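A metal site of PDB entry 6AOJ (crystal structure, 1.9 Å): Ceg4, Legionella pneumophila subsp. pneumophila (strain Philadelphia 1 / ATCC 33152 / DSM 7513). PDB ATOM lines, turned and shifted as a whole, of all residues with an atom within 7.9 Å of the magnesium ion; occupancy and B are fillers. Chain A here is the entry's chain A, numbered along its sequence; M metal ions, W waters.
Three residues have an atom within 4 Å of the magnesium ion: Asp 15, Asp 17 and Asp 164.
N of Asp 164 is in hydrogen-bond range of OG1 of Thr 19, 3.1 Å away.
The side-chain hydroxyl (OG1) of Thr 19 lies close to the side-chain carboxylate (OD2) of Asp 15.
OD1 of Asp 15 is in salt-bridge range of NZ of Lys 141.
The backbone NH (N) of Asp 15 lies within hydrogen-bond range of the backbone carbonyl oxygen (O) of Leu 162 (2.9 Å).
Water W2 bridges OD1 of Asp 163 (2.7 Å) and OD1 of Asp 15 (3.5 Å).
Water W1 lies within hydrogen-bond range of the side-chain carboxylate of Asp 164 (2.5 Å) and the backbone NH of Gly 25 (3.2 Å).
The magnesium ion is bound by water W3, the side-chain carboxylate of Asp 164, the backbone carbonyl oxygen of Asp 17, the side-chain carboxylate of Asp 15, water W2 and water W1.
The magnesium ion has six donor atoms within binding distance.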
ATOM      1  N   ASP A  15     -20.636  20.165  25.266  1.00  0.00           N
ATOM      2  CA  ASP A  15     -21.417  18.993  24.921  1.00  0.00           C
ATOM      3  C   ASP A  15     -22.856  19.206  25.398  1.00  0.00           C
ATOM      4  O   ASP A  15     -23.131  20.113  26.208  1.00  0.00           O
ATOM      5  CB  ASP A  15     -20.769  17.769  25.561  1.00  0.00           C
ATOM      6  CG  ASP A  15     -21.561  16.489  25.332  1.00  0.00           C
ATOM      7  OD1 ASP A  15     -21.858  16.195  24.156  1.00  0.00           O
ATOM      8  OD2 ASP A  15     -21.859  15.777  26.328  1.00  0.00           O
ATOM      9  N   PHE A  16     -23.793  18.409  24.871  1.00  0.00           N
ATOM     10  CA  PHE A  16     -25.176  18.501  25.326  1.00  0.00           C
ATOM     11  C   PHE A  16     -25.535  17.319  26.227  1.00  0.00           C
ATOM     12  O   PHE A  16     -25.728  17.491  27.436  1.00  0.00           O
ATOM     13  CB  PHE A  16     -26.144  18.601  24.148  1.00  0.00           C
ATOM     14  CG  PHE A  16     -27.580  18.757  24.568  1.00  0.00           C
ATOM     15  CD1 PHE A  16     -28.058  19.999  25.008  1.00  0.00           C
ATOM     16  CD2 PHE A  16     -28.439  17.677  24.528  1.00  0.00           C
ATOM     17  CE1 PHE A  16     -29.405  20.158  25.393  1.00  0.00           C
ATOM     18  CE2 PHE A  16     -29.772  17.810  24.920  1.00  0.00           C
ATOM     19  CZ  PHE A  16     -30.251  19.046  25.347  1.00  0.00           C
ATOM     20  N   ASP A  17     -25.623  16.108  25.647  1.00  0.00           N
ATOM     21  CA  ASP A  17     -26.084  14.948  26.408  1.00  0.00           C
ATOM     22  C   ASP A  17     -25.059  14.497  27.440  1.00  0.00           C
ATOM     23  O   ASP A  17     -23.939  14.099  27.085  1.00  0.00           O
ATOM     24  CB  ASP A  17     -26.381  13.758  25.477  1.00  0.00           C
ATOM     25  CG  ASP A  17     -27.515  14.046  24.496  1.00  0.00           C
ATOM     26  OD1 ASP A  17     -28.689  14.261  24.929  1.00  0.00           O
ATOM     27  OD2 ASP A  17     -27.211  14.032  23.288  1.00  0.00           O
ATOM     28  N   GLY A  18     -25.451  14.478  28.708  1.00  0.00           N
ATOM     29  CA  GLY A  18     -24.585  14.071  29.774  1.00  0.00           C
ATOM     30  C   GLY A  18     -23.750  15.195  30.348  1.00  0.00           C
ATOM     31  O   GLY A  18     -23.076  14.994  31.359  1.00  0.00           O
ATOM     32  N   THR A  19     -23.822  16.382  29.755  1.00  0.00           N
ATOM     33  CA  THR A  19     -23.111  17.578  30.209  1.00  0.00           C
ATOM     34  C   THR A  19     -24.124  18.646  30.605  1.00  0.00           C
ATOM     35  O   THR A  19     -24.193  19.014  31.784  1.00  0.00           O
ATOM     36  CB  THR A  19     -22.195  18.074  29.084  1.00  0.00           C
ATOM     37  OG1 THR A  19     -21.229  17.045  28.805  1.00  0.00           O
ATOM     38  CG2 THR A  19     -21.460  19.402  29.441  1.00  0.00           C
ATOM     39  N   VAL A  20     -24.921  19.098  29.658  1.00  0.00           N
ATOM     40  CA  VAL A  20     -26.054  19.971  29.969  1.00  0.00           C
ATOM     41  C   VAL A  20     -27.200  19.151  30.564  1.00  0.00           C
ATOM     42  O   VAL A  20     -27.763  19.540  31.591  1.00  0.00           O
ATOM     43  CB  VAL A  20     -26.467  20.730  28.703  1.00  0.00           C
ATOM     44  CG1 VAL A  20     -27.765  21.559  28.919  1.00  0.00           C
ATOM     45  CG2 VAL A  20     -25.345  21.665  28.271  1.00  0.00           C
ATOM     46  N   THR A  21     -27.514  17.986  29.984  1.00  0.00           N
ATOM     47  CA  THR A  21     -28.414  17.006  30.625  1.00  0.00           C
ATOM     48  C   THR A  21     -27.666  16.033  31.529  1.00  0.00           C
ATOM     49  O   THR A  21     -26.439  15.975  31.558  1.00  0.00           O
ATOM     50  CB  THR A  21     -29.170  16.178  29.587  1.00  0.00           C
ATOM     51  OG1 THR A  21     -28.318  15.128  29.102  1.00  0.00           O
ATOM     52  CG2 THR A  21     -29.608  17.053  28.411  1.00  0.00           C
ATOM     53  N   LYS A  23     -27.866  12.706  31.290  1.00  0.00           N
ATOM     54  CA  LYS A  23     -27.785  11.353  30.746  1.00  0.00           C
ATOM     55  C   LYS A  23     -26.824  11.331  29.577  1.00  0.00           C
ATOM     56  O   LYS A  23     -26.773  12.292  28.800  1.00  0.00           O
ATOM     57  CB  LYS A  23     -29.174  10.868  30.300  1.00  0.00           C
ATOM     58  CG  LYS A  23     -30.069  10.426  31.443  1.00  0.00           C
ATOM     59  CD  LYS A  23     -29.786   8.980  31.838  1.00  0.00           C
ATOM     60  CE  LYS A  23     -29.863   8.803  33.344  1.00  0.00           C
ATOM     61  NZ  LYS A  23     -30.334   7.444  33.714  1.00  0.00           N
ATOM     62  N   SER A  24     -26.059  10.264  29.417  1.00  0.00           N
ATOM     63  CA  SER A  24     -25.128  10.267  28.291  1.00  0.00           C
ATOM     64  C   SER A  24     -25.907  10.137  26.972  1.00  0.00           C
ATOM     65  O   SER A  24     -27.035   9.655  26.934  1.00  0.00           O
ATOM     66  CB  SER A  24     -24.090   9.157  28.436  1.00  0.00           C
ATOM     67  OG  SER A  24     -24.685   7.892  28.164  1.00  0.00           O
ATOM     68  N   GLY A  25     -25.270  10.572  25.883  1.00  0.00           N
ATOM     69  CA  GLY A  25     -25.927  10.484  24.588  1.00  0.00           C
ATOM     70  C   GLY A  25     -26.287   9.066  24.205  1.00  0.00           C
ATOM     71  O   GLY A  25     -27.390   8.793  23.712  1.00  0.00           O
ATOM     72  N   ASN A  26     -25.370   8.107  24.461  1.00  0.00           N
ATOM     73  CA  ASN A  26     -25.656   6.721  24.133  1.00  0.00           C
ATOM     74  C   ASN A  26     -26.837   6.206  24.939  1.00  0.00           C
ATOM     75  O   ASN A  26     -27.497   5.243  24.526  1.00  0.00           O
ATOM     76  CB  ASN A  26     -24.436   5.818  24.388  1.00  0.00           C
ATOM     77  CG  ASN A  26     -23.268   6.130  23.452  1.00  0.00           C
ATOM     78  OD1 ASN A  26     -23.451   6.430  22.277  1.00  0.00           O
ATOM     79  ND2 ASN A  26     -22.051   6.037  23.985  1.00  0.00           N
ATOM     80  N   VAL A 108     -21.682  21.356  20.880  1.00  0.00           N
ATOM     81  CA  VAL A 108     -20.927  20.497  19.975  1.00  0.00           C
ATOM     82  C   VAL A 108     -21.337  19.073  20.307  1.00  0.00           C
ATOM     83  O   VAL A 108     -21.076  18.585  21.416  1.00  0.00           O
ATOM     84  CB  VAL A 108     -19.408  20.689  20.136  1.00  0.00           C
ATOM     85  CG1 VAL A 108     -18.659  19.928  19.056  1.00  0.00           C
ATOM     86  CG2 VAL A 108     -19.061  22.191  20.044  1.00  0.00           C
ATOM     87  N   THR A 109     -21.992  18.401  19.352  1.00  0.00           N
ATOM     88  CA  THR A 109     -22.856  17.303  19.726  1.00  0.00           C
ATOM     89  C   THR A 109     -22.935  16.240  18.618  1.00  0.00           C
ATOM     90  O   THR A 109     -22.774  16.546  17.436  1.00  0.00           O
ATOM     91  CB  THR A 109     -24.268  17.830  20.102  1.00  0.00           C
ATOM     92  OG1 THR A 109     -25.064  16.742  20.608  1.00  0.00           O
ATOM     93  CG2 THR A 109     -24.994  18.492  18.909  1.00  0.00           C
ATOM     94  N   LYS A 110     -23.138  14.976  19.022  1.00  0.00           N
ATOM     95  CA  LYS A 110     -23.578  13.952  18.066  1.00  0.00           C
ATOM     96  C   LYS A 110     -25.089  13.823  18.039  1.00  0.00           C
ATOM     97  O   LYS A 110     -25.618  12.980  17.314  1.00  0.00           O
ATOM     98  CB  LYS A 110     -22.991  12.578  18.402  1.00  0.00           C
ATOM     99  CG  LYS A 110     -21.479  12.526  18.150  1.00  0.00           C
ATOM    100  CD  LYS A 110     -20.991  11.206  18.723  1.00  0.00           C
ATOM    101  CE  LYS A 110     -19.815  11.428  19.616  1.00  0.00           C
ATOM    102  NZ  LYS A 110     -18.578  11.174  18.848  1.00  0.00           N
ATOM    103  N   LYS A 141     -15.834  16.386  16.611  1.00  0.00           N
ATOM    104  CA  LYS A 141     -15.784  17.556  17.489  1.00  0.00           C
ATOM    105  C   LYS A 141     -14.522  18.379  17.296  1.00  0.00           C
ATOM    106  O   LYS A 141     -14.571  19.621  17.449  1.00  0.00           O
ATOM    107  CB  LYS A 141     -15.938  17.130  18.956  1.00  0.00           C
ATOM    108  CG  LYS A 141     -17.322  16.592  19.276  1.00  0.00           C
ATOM    109  CD  LYS A 141     -17.750  16.784  20.750  1.00  0.00           C
ATOM    110  CE  LYS A 141     -19.013  15.922  21.038  1.00  0.00           C
ATOM    111  NZ  LYS A 141     -19.599  16.244  22.369  1.00  0.00           N
ATOM    112  N   LEU A 162     -16.524  21.900  27.920  1.00  0.00           N
ATOM    113  CA  LEU A 162     -17.248  21.014  28.830  1.00  0.00           C
ATOM    114  C   LEU A 162     -17.666  19.755  28.069  1.00  0.00           C
ATOM    115  O   LEU A 162     -18.342  19.856  27.041  1.00  0.00           O
ATOM    116  CB  LEU A 162     -18.495  21.724  29.402  1.00  0.00           C
ATOM    117  CG  LEU A 162     -18.223  23.029  30.180  1.00  0.00           C
ATOM    118  CD1 LEU A 162     -18.440  24.264  29.352  1.00  0.00           C
ATOM    119  CD2 LEU A 162     -19.015  23.127  31.476  1.00  0.00           C
ATOM    120  N   ASP A 163     -17.268  18.577  28.557  1.00  0.00           N
ATOM    121  CA  ASP A 163     -17.764  17.360  27.918  1.00  0.00           C
ATOM    122  C   ASP A 163     -17.644  16.193  28.904  1.00  0.00           C
ATOM    123  O   ASP A 163     -16.633  16.062  29.598  1.00  0.00           O
ATOM    124  CB  ASP A 163     -16.996  17.076  26.621  1.00  0.00           C
ATOM    125  CG  ASP A 163     -17.763  16.155  25.651  1.00  0.00           C
ATOM    126  OD1 ASP A 163     -18.284  15.094  26.091  1.00  0.00           O
ATOM    127  OD2 ASP A 163     -17.841  16.487  24.441  1.00  0.00           O
ATOM    128  N   ASP A 164     -18.701  15.342  28.981  1.00  0.00           N
ATOM    129  CA  ASP A 164     -18.627  14.184  29.866  1.00  0.00           C
ATOM    130  C   ASP A 164     -17.801  13.056  29.270  1.00  0.00           C
ATOM    131  O   ASP A 164     -17.324  12.165  30.019  1.00  0.00           O
ATOM    132  CB  ASP A 164     -20.040  13.631  30.218  1.00  0.00           C
ATOM    133  CG  ASP A 164     -20.840  13.203  28.983  1.00  0.00           C
ATOM    134  OD1 ASP A 164     -20.983  14.012  28.067  1.00  0.00           O
ATOM    135  OD2 ASP A 164     -21.370  12.047  28.901  1.00  0.00           O
ATOM    136  N   SER A 165     -17.642  13.029  27.957  1.00  0.00           N
ATOM    137  CA  SER A 165     -16.857  11.966  27.319  1.00  0.00           C
ATOM    138  C   SER A 165     -15.378  12.311  27.356  1.00  0.00           C
ATOM    139  O   SER A 165     -14.983  13.347  26.802  1.00  0.00           O
ATOM    140  CB  SER A 165     -17.285  11.803  25.869  1.00  0.00           C
ATOM    141  OG  SER A 165     -16.225  11.209  25.113  1.00  0.00           O
ATOM    142  N   ASP A 168     -14.043  12.837  23.615  1.00  0.00           N
ATOM    143  CA  ASP A 168     -14.582  14.005  22.908  1.00  0.00           C
ATOM    144  C   ASP A 168     -14.140  15.304  23.558  1.00  0.00           C
ATOM    145  O   ASP A 168     -13.835  16.283  22.867  1.00  0.00           O
ATOM    146  CB  ASP A 168     -16.101  13.903  22.833  1.00  0.00           C
ATOM    147  CG  ASP A 168     -16.536  12.948  21.718  1.00  0.00           C
ATOM    148  OD1 ASP A 168     -15.799  12.852  20.697  1.00  0.00           O
ATOM    149  OD2 ASP A 168     -17.562  12.268  21.878  1.00  0.00           O
ATOM    150  N   LYS A 191     -16.292  16.087  33.373  1.00  0.00           N
ATOM    151  CA  LYS A 191     -17.016  15.590  34.544  1.00  0.00           C
ATOM    152  C   LYS A 191     -17.968  14.487  34.122  1.00  0.00           C
ATOM    153  O   LYS A 191     -18.405  14.440  32.964  1.00  0.00           O
ATOM    154  CB  LYS A 191     -17.803  16.757  35.231  1.00  0.00           C
ATOM    155  CG  LYS A 191     -16.949  18.006  35.557  1.00  0.00           C
ATOM    156  CD  LYS A 191     -15.952  17.666  36.698  1.00  0.00           C
ATOM    157  CE  LYS A 191     -14.899  18.753  36.862  1.00  0.00           C
ATOM    158  NZ  LYS A 191     -14.099  18.501  38.094  1.00  0.00           N
ATOM    159  N   PRO A 193     -21.705  12.617  34.071  1.00  0.00           N
ATOM    160  CA  PRO A 193     -23.039  13.225  33.989  1.00  0.00           C
ATOM    161  C   PRO A 193     -23.597  13.560  35.361  1.00  0.00           C
ATOM    162  O   PRO A 193     -23.559  12.740  36.276  1.00  0.00           O
ATOM    163  CB  PRO A 193     -23.865  12.122  33.307  1.00  0.00           C
ATOM    164  CG  PRO A 193     -22.895  11.413  32.461  1.00  0.00           C
ATOM    165  CD  PRO A 193     -21.589  11.422  33.228  1.00  0.00           C
ATOM    166  N   PHE A 196     -21.314  18.322  36.830  1.00  0.00           N
ATOM    167  CA  PHE A 196     -20.811  19.643  36.457  1.00  0.00           C
ATOM    168  C   PHE A 196     -21.323  20.686  37.436  1.00  0.00           C
ATOM    169  O   PHE A 196     -22.382  20.526  38.044  1.00  0.00           O
ATOM    170  CB  PHE A 196     -21.236  20.015  35.033  1.00  0.00           C
ATOM    171  CG  PHE A 196     -20.560  19.178  33.971  1.00  0.00           C
ATOM    172  CD1 PHE A 196     -21.086  17.938  33.605  1.00  0.00           C
ATOM    173  CD2 PHE A 196     -19.389  19.633  33.368  1.00  0.00           C
ATOM    174  CE1 PHE A 196     -20.446  17.167  32.627  1.00  0.00           C
ATOM    175  CE2 PHE A 196     -18.737  18.876  32.407  1.00  0.00           C
ATOM    176  CZ  PHE A 196     -19.270  17.634  32.018  1.00  0.00           C
HETATM  177 MG    MG M   1     -22.057  13.695  26.336  1.00  0.00          MG
HETATM  178  O   HOH W   1     -22.366  11.614  26.661  1.00  0.00           O
HETATM  179  O   HOH W   2     -20.194  13.394  25.370  1.00  0.00           O
HETATM  180  O   HOH W   3     -22.762  13.410  24.464  1.00  0.00           O
